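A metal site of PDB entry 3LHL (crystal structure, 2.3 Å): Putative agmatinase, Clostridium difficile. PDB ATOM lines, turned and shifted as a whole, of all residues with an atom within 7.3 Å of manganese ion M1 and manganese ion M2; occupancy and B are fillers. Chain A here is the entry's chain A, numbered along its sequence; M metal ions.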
ATOM      1  N   GLU A  97       2.014  -9.527  21.511  1.00  0.00           N
ATOM      2  CA  GLU A  97       0.816  -8.922  20.943  1.00  0.00           C
ATOM      3  C   GLU A  97      -0.496  -9.489  21.493  1.00  0.00           C
ATOM      4  O   GLU A  97      -0.548 -10.585  22.049  1.00  0.00           O
ATOM      5  CB  GLU A  97       0.821  -9.028  19.420  1.00  0.00           C
ATOM      6  CG  GLU A  97       0.744 -10.417  18.886  1.00  0.00           C
ATOM      7  CD  GLU A  97       0.656 -10.425  17.375  1.00  0.00           C
ATOM      8  OE1 GLU A  97       1.625  -9.966  16.719  1.00  0.00           O
ATOM      9  OE2 GLU A  97      -0.382 -10.876  16.846  1.00  0.00           O
ATOM     10  N   HIS A  98      -1.558  -8.706  21.315  1.00  0.00           N
ATOM     11  CA  HIS A  98      -2.869  -9.074  21.838  1.00  0.00           C
ATOM     12  C   HIS A  98      -3.500 -10.322  21.215  1.00  0.00           C
ATOM     13  O   HIS A  98      -4.423 -10.899  21.771  1.00  0.00           O
ATOM     14  CB  HIS A  98      -3.813  -7.888  21.715  1.00  0.00           C
ATOM     15  CG  HIS A  98      -4.804  -7.783  22.833  1.00  0.00           C
ATOM     16  ND1 HIS A  98      -5.533  -6.639  23.089  1.00  0.00           N
ATOM     17  CD2 HIS A  98      -5.192  -8.697  23.758  1.00  0.00           C
ATOM     18  CE1 HIS A  98      -6.320  -6.846  24.132  1.00  0.00           C
ATOM     19  NE2 HIS A  98      -6.132  -8.082  24.557  1.00  0.00           N
ATOM     20  N   LEU A  99      -3.002 -10.752  20.062  1.00  0.00           N
ATOM     21  CA  LEU A  99      -3.600 -11.926  19.432  1.00  0.00           C
ATOM     22  C   LEU A  99      -3.466 -13.193  20.288  1.00  0.00           C
ATOM     23  O   LEU A  99      -4.324 -14.073  20.213  1.00  0.00           O
ATOM     24  CB  LEU A  99      -2.985 -12.163  18.045  1.00  0.00           C
ATOM     25  CG  LEU A  99      -3.607 -13.293  17.211  1.00  0.00           C
ATOM     26  CD1 LEU A  99      -5.106 -13.073  17.039  1.00  0.00           C
ATOM     27  CD2 LEU A  99      -2.909 -13.355  15.867  1.00  0.00           C
ATOM     28  N   HIS A 119     -12.266  -6.304  29.150  1.00  0.00           N
ATOM     29  CA  HIS A 119     -11.237  -5.827  28.240  1.00  0.00           C
ATOM     30  C   HIS A 119     -10.742  -4.388  28.474  1.00  0.00           C
ATOM     31  O   HIS A 119     -11.516  -3.438  28.359  1.00  0.00           O
ATOM     32  CB  HIS A 119     -11.794  -5.987  26.820  1.00  0.00           C
ATOM     33  CG  HIS A 119     -10.940  -5.407  25.725  1.00  0.00           C
ATOM     34  ND1 HIS A 119      -9.625  -5.779  25.533  1.00  0.00           N
ATOM     35  CD2 HIS A 119     -11.242  -4.548  24.733  1.00  0.00           C
ATOM     36  CE1 HIS A 119      -9.164  -5.167  24.453  1.00  0.00           C
ATOM     37  NE2 HIS A 119     -10.116  -4.414  23.950  1.00  0.00           N
ATOM     38  N   PHE A 120      -9.464  -4.244  28.803  1.00  0.00           N
ATOM     39  CA  PHE A 120      -8.850  -2.929  29.020  1.00  0.00           C
ATOM     40  C   PHE A 120      -7.951  -2.681  27.819  1.00  0.00           C
ATOM     41  O   PHE A 120      -7.126  -3.524  27.456  1.00  0.00           O
ATOM     42  CB  PHE A 120      -8.040  -2.917  30.316  1.00  0.00           C
ATOM     43  CG  PHE A 120      -8.889  -2.789  31.556  1.00  0.00           C
ATOM     44  CD1 PHE A 120      -9.318  -1.535  31.989  1.00  0.00           C
ATOM     45  CD2 PHE A 120      -9.283  -3.911  32.263  1.00  0.00           C
ATOM     46  CE1 PHE A 120     -10.138  -1.409  33.115  1.00  0.00           C
ATOM     47  CE2 PHE A 120     -10.104  -3.795  33.393  1.00  0.00           C
ATOM     48  CZ  PHE A 120     -10.530  -2.546  33.813  1.00  0.00           C
ATOM     49  N   ASP A 121      -8.094  -1.518  27.206  1.00  0.00           N
ATOM     50  CA  ASP A 121      -7.324  -1.238  25.995  1.00  0.00           C
ATOM     51  C   ASP A 121      -7.496   0.222  25.573  1.00  0.00           C
ATOM     52  O   ASP A 121      -8.449   0.899  25.977  1.00  0.00           O
ATOM     53  CB  ASP A 121      -7.862  -2.126  24.864  1.00  0.00           C
ATOM     54  CG  ASP A 121      -6.808  -2.509  23.843  1.00  0.00           C
ATOM     55  OD1 ASP A 121      -6.133  -1.613  23.284  1.00  0.00           O
ATOM     56  OD2 ASP A 121      -6.659  -3.731  23.594  1.00  0.00           O
ATOM     57  N   ALA A 122      -6.565   0.705  24.760  1.00  0.00           N
ATOM     58  CA  ALA A 122      -6.640   2.056  24.236  1.00  0.00           C
ATOM     59  C   ALA A 122      -7.379   1.922  22.903  1.00  0.00           C
ATOM     60  O   ALA A 122      -7.987   2.883  22.415  1.00  0.00           O
ATOM     61  CB  ALA A 122      -5.255   2.607  23.998  1.00  0.00           C
ATOM     62  N   HIS A 123      -7.335   0.711  22.353  1.00  0.00           N
ATOM     63  CA  HIS A 123      -7.974   0.403  21.079  1.00  0.00           C
ATOM     64  C   HIS A 123      -9.151  -0.567  21.208  1.00  0.00           C
ATOM     65  O   HIS A 123      -9.157  -1.441  22.080  1.00  0.00           O
ATOM     66  CB  HIS A 123      -6.940  -0.176  20.112  1.00  0.00           C
ATOM     67  CG  HIS A 123      -5.656   0.579  20.096  1.00  0.00           C
ATOM     68  ND1 HIS A 123      -4.625   0.308  20.970  1.00  0.00           N
ATOM     69  CD2 HIS A 123      -5.263   1.658  19.371  1.00  0.00           C
ATOM     70  CE1 HIS A 123      -3.650   1.193  20.792  1.00  0.00           C
ATOM     71  NE2 HIS A 123      -4.014   2.025  19.833  1.00  0.00           N
ATOM     72  N   THR A 124     -10.128  -0.420  20.312  1.00  0.00           N
ATOM     73  CA  THR A 124     -11.310  -1.267  20.306  1.00  0.00           C
ATOM     74  C   THR A 124     -10.981  -2.713  19.933  1.00  0.00           C
ATOM     75  O   THR A 124     -11.514  -3.658  20.513  1.00  0.00           O
ATOM     76  CB  THR A 124     -12.380  -0.751  19.294  1.00  0.00           C
ATOM     77  OG1 THR A 124     -11.932  -0.992  17.955  1.00  0.00           O
ATOM     78  CG2 THR A 124     -12.638   0.751  19.493  1.00  0.00           C
ATOM     79  N   ASP A 125     -10.090  -2.882  18.948  1.00  0.00           N
ATOM     80  CA  ASP A 125      -9.721  -4.211  18.476  1.00  0.00           C
ATOM     81  C   ASP A 125     -10.948  -4.924  17.879  1.00  0.00           C
ATOM     82  O   ASP A 125     -11.009  -6.145  17.843  1.00  0.00           O
ATOM     83  CB  ASP A 125      -9.152  -5.057  19.622  1.00  0.00           C
ATOM     84  CG  ASP A 125      -7.727  -4.660  19.976  1.00  0.00           C
ATOM     85  OD1 ASP A 125      -7.135  -3.855  19.228  1.00  0.00           O
ATOM     86  OD2 ASP A 125      -7.214  -5.153  20.998  1.00  0.00           O
ATOM     87  N   HIS A 137      -3.633  -8.587  16.118  1.00  0.00           N
ATOM     88  CA  HIS A 137      -3.774  -8.034  17.452  1.00  0.00           C
ATOM     89  C   HIS A 137      -4.913  -7.011  17.459  1.00  0.00           C
ATOM     90  O   HIS A 137      -5.549  -6.773  18.487  1.00  0.00           O
ATOM     91  CB  HIS A 137      -2.470  -7.338  17.905  1.00  0.00           C
ATOM     92  CG  HIS A 137      -1.978  -6.293  16.960  1.00  0.00           C
ATOM     93  ND1 HIS A 137      -1.171  -6.575  15.878  1.00  0.00           N
ATOM     94  CD2 HIS A 137      -2.152  -4.946  16.941  1.00  0.00           C
ATOM     95  CE1 HIS A 137      -0.874  -5.462  15.236  1.00  0.00           C
ATOM     96  NE2 HIS A 137      -1.461  -4.452  15.863  1.00  0.00           N
ATOM     97  N   ALA A 138      -5.188  -6.434  16.284  1.00  0.00           N
ATOM     98  CA  ALA A 138      -6.232  -5.417  16.129  1.00  0.00           C
ATOM     99  C   ALA A 138      -7.647  -5.932  15.876  1.00  0.00           C
ATOM    100  O   ALA A 138      -8.593  -5.141  15.765  1.00  0.00           O
ATOM    101  CB  ALA A 138      -5.834  -4.453  15.012  1.00  0.00           C
ATOM    102  N   VAL A 140      -8.603  -8.999  17.601  1.00  0.00           N
ATOM    103  CA  VAL A 140      -8.815  -9.979  18.652  1.00  0.00           C
ATOM    104  C   VAL A 140     -10.197  -9.966  19.332  1.00  0.00           C
ATOM    105  O   VAL A 140     -10.792 -11.022  19.528  1.00  0.00           O
ATOM    106  CB  VAL A 140      -7.698  -9.902  19.738  1.00  0.00           C
ATOM    107  CG1 VAL A 140      -7.824  -8.612  20.554  1.00  0.00           C
ATOM    108  CG2 VAL A 140      -7.768 -11.129  20.636  1.00  0.00           C
ATOM    109  N   ILE A 141     -10.706  -8.788  19.673  1.00  0.00           N
ATOM    110  CA  ILE A 141     -12.007  -8.744  20.330  1.00  0.00           C
ATOM    111  C   ILE A 141     -13.148  -9.118  19.388  1.00  0.00           C
ATOM    112  O   ILE A 141     -14.156  -9.679  19.813  1.00  0.00           O
ATOM    113  CB  ILE A 141     -12.276  -7.347  20.949  1.00  0.00           C
ATOM    114  CG1 ILE A 141     -11.193  -7.043  21.995  1.00  0.00           C
ATOM    115  CG2 ILE A 141     -13.651  -7.313  21.628  1.00  0.00           C
ATOM    116  CD1 ILE A 141     -11.083  -8.096  23.077  1.00  0.00           C
ATOM    117  N   THR A 200      -8.586  -9.664  30.110  1.00  0.00           N
ATOM    118  CA  THR A 200      -7.519  -9.374  29.165  1.00  0.00           C
ATOM    119  C   THR A 200      -7.164  -7.895  29.245  1.00  0.00           C
ATOM    120  O   THR A 200      -7.982  -7.017  28.957  1.00  0.00           O
ATOM    121  CB  THR A 200      -7.913  -9.738  27.704  1.00  0.00           C
ATOM    122  OG1 THR A 200      -6.833  -9.381  26.825  1.00  0.00           O
ATOM    123  CG2 THR A 200      -9.188  -9.011  27.285  1.00  0.00           C
ATOM    124  N   ILE A 201      -5.926  -7.627  29.641  1.00  0.00           N
ATOM    125  CA  ILE A 201      -5.447  -6.263  29.789  1.00  0.00           C
ATOM    126  C   ILE A 201      -4.368  -5.868  28.786  1.00  0.00           C
ATOM    127  O   ILE A 201      -3.232  -6.357  28.864  1.00  0.00           O
ATOM    128  CB  ILE A 201      -4.896  -6.022  31.215  1.00  0.00           C
ATOM    129  CG1 ILE A 201      -6.046  -6.055  32.224  1.00  0.00           C
ATOM    130  CG2 ILE A 201      -4.135  -4.694  31.287  1.00  0.00           C
ATOM    131  CD1 ILE A 201      -5.603  -5.871  33.663  1.00  0.00           C
ATOM    132  N   ASP A 202      -4.729  -5.009  27.837  1.00  0.00           N
ATOM    133  CA  ASP A 202      -3.757  -4.500  26.875  1.00  0.00           C
ATOM    134  C   ASP A 202      -3.127  -3.336  27.645  1.00  0.00           C
ATOM    135  O   ASP A 202      -3.820  -2.367  27.957  1.00  0.00           O
ATOM    136  CB  ASP A 202      -4.440  -3.983  25.621  1.00  0.00           C
ATOM    137  CG  ASP A 202      -3.459  -3.448  24.599  1.00  0.00           C
ATOM    138  OD1 ASP A 202      -2.500  -2.771  25.014  1.00  0.00           O
ATOM    139  OD2 ASP A 202      -3.647  -3.701  23.400  1.00  0.00           O
ATOM    140  N   LEU A 203      -1.848  -3.439  27.971  1.00  0.00           N
ATOM    141  CA  LEU A 203      -1.183  -2.397  28.745  1.00  0.00           C
ATOM    142  C   LEU A 203      -1.209  -0.992  28.131  1.00  0.00           C
ATOM    143  O   LEU A 203      -0.990  -0.020  28.848  1.00  0.00           O
ATOM    144  CB  LEU A 203       0.250  -2.807  29.071  1.00  0.00           C
ATOM    145  CG  LEU A 203       0.367  -4.077  29.941  1.00  0.00           C
ATOM    146  CD1 LEU A 203       1.809  -4.528  30.024  1.00  0.00           C
ATOM    147  CD2 LEU A 203      -0.193  -3.794  31.332  1.00  0.00           C
ATOM    148  N   ASP A 204      -1.471  -0.871  26.825  1.00  0.00           N
ATOM    149  CA  ASP A 204      -1.511   0.472  26.265  1.00  0.00           C
ATOM    150  C   ASP A 204      -2.781   1.214  26.690  1.00  0.00           C
ATOM    151  O   ASP A 204      -3.056   2.308  26.198  1.00  0.00           O
ATOM    152  CB  ASP A 204      -1.394   0.468  24.730  1.00  0.00           C
ATOM    153  CG  ASP A 204      -2.569  -0.179  24.022  1.00  0.00           C
ATOM    154  OD1 ASP A 204      -3.696  -0.184  24.571  1.00  0.00           O
ATOM    155  OD2 ASP A 204      -2.362  -0.681  22.909  1.00  0.00           O
ATOM    156  N   VAL A 205      -3.549   0.624  27.591  1.00  0.00           N
ATOM    157  CA  VAL A 205      -4.735   1.301  28.092  1.00  0.00           C
ATOM    158  C   VAL A 205      -4.212   2.485  28.894  1.00  0.00           C
ATOM    159  O   VAL A 205      -4.879   3.505  29.040  1.00  0.00           O
ATOM    160  CB  VAL A 205      -5.589   0.387  29.008  1.00  0.00           C
ATOM    161  CG1 VAL A 205      -4.848   0.070  30.311  1.00  0.00           C
ATOM    162  CG2 VAL A 205      -6.925   1.056  29.304  1.00  0.00           C
ATOM    163  N   THR A 214       5.223   0.432  24.232  1.00  0.00           N
ATOM    164  CA  THR A 214       4.152  -0.346  23.627  1.00  0.00           C
ATOM    165  C   THR A 214       4.109  -0.067  22.135  1.00  0.00           C
ATOM    166  O   THR A 214       4.639   0.948  21.671  1.00  0.00           O
ATOM    167  CB  THR A 214       2.792  -0.019  24.291  1.00  0.00           C
ATOM    168  OG1 THR A 214       1.822  -1.012  23.911  1.00  0.00           O
ATOM    169  CG2 THR A 214       2.292   1.348  23.839  1.00  0.00           C
ATOM    170  N   THR A 216       1.504   0.702  19.888  1.00  0.00           N
ATOM    171  CA  THR A 216       0.694   1.801  19.370  1.00  0.00           C
ATOM    172  C   THR A 216       0.246   2.746  20.485  1.00  0.00           C
ATOM    173  O   THR A 216      -0.911   2.745  20.881  1.00  0.00           O
ATOM    174  CB  THR A 216      -0.570   1.237  18.691  1.00  0.00           C
ATOM    175  OG1 THR A 216      -0.216   0.065  17.968  1.00  0.00           O
ATOM    176  CG2 THR A 216      -1.186   2.274  17.745  1.00  0.00           C
ATOM    177  N   VAL A 247      -0.901  -7.751  27.980  1.00  0.00           N
ATOM    178  CA  VAL A 247      -0.203  -7.800  26.709  1.00  0.00           C
ATOM    179  C   VAL A 247       0.235  -6.450  26.172  1.00  0.00           C
ATOM    180  O   VAL A 247      -0.110  -5.409  26.720  1.00  0.00           O
ATOM    181  CB  VAL A 247      -1.109  -8.470  25.634  1.00  0.00           C
ATOM    182  CG1 VAL A 247      -1.468  -9.897  26.042  1.00  0.00           C
ATOM    183  CG2 VAL A 247      -2.381  -7.650  25.449  1.00  0.00           C
ATOM    184  N   GLU A 248       1.002  -6.511  25.083  1.00  0.00           N
ATOM    185  CA  GLU A 248       1.489  -5.342  24.364  1.00  0.00           C
ATOM    186  C   GLU A 248       2.636  -4.539  24.980  1.00  0.00           C
ATOM    187  O   GLU A 248       2.924  -3.415  24.541  1.00  0.00           O
ATOM    188  CB  GLU A 248       0.306  -4.419  24.010  1.00  0.00           C
ATOM    189  CG  GLU A 248      -0.682  -5.055  23.021  1.00  0.00           C
ATOM    190  CD  GLU A 248      -0.045  -5.450  21.678  1.00  0.00           C
ATOM    191  OE1 GLU A 248       1.196  -5.517  21.599  1.00  0.00           O
ATOM    192  OE2 GLU A 248      -0.791  -5.707  20.703  1.00  0.00           O
HETATM  193 MN    MN M   1      -5.263  -4.625  22.192  1.00  0.00          MN
HETATM  194 MN    MN M   2      -4.047  -1.645  22.294  1.00  0.00          MN
HETATM  195 MN    MN M   3      -3.563  -3.815  20.039  1.00  0.00          MN
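A ring nitrogen (NE2) of His 98 is in hydrogen-bond range of the side-chain hydroxyl (OG1) of Thr 200. The backbone NH (N) of His 98 lies within hydrogen-bond range of the side-chain carboxylate (OE2) of Glu 248 (3.2 Å). The backbone carbonyl oxygen (O) of Asp 125 sits at hydrogen-bond distance from the backbone NH (N) of Ile 141, 3.2 Å away. N of Asp 202 is in hydrogen-bond range of O of Phe 120 (2.8 Å). The side-chain carboxylate of Asp 204 sits at hydrogen-bond distance from the backbone NH of Ala 122 (3.0 Å). The backbone carbonyl oxygen of Thr 216 lies close to a ring nitrogen (NE2) of His 123 (3.4 Å).
Manganese ion M1 is bound by the side-chain carboxylate of Asp 121 (2.2 Å), the side-chain carboxylate of Asp 202 (2.2 Å), a ring nitrogen (ND1) of His 98 (2.2 Å) and the side-chain carboxylate of Asp 125 (2.3 Å).
Of the 24 residues printed, 4 come within 4 Å of manganese ion M2.
Manganese ion M2 is bound by the side-chain carboxylate of Asp 204 (2.0 Å), the side-chain carboxylate of Asp 121 (2.3 Å), the side-chain carboxylate of Asp 202 (2.4 Å) and a ring nitrogen (ND1) of His 123 (2.4 Å). Slightly farther from manganese ion M2 lies the side-chain carboxylate (OD1) of Asp 204 (2.7 Å).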
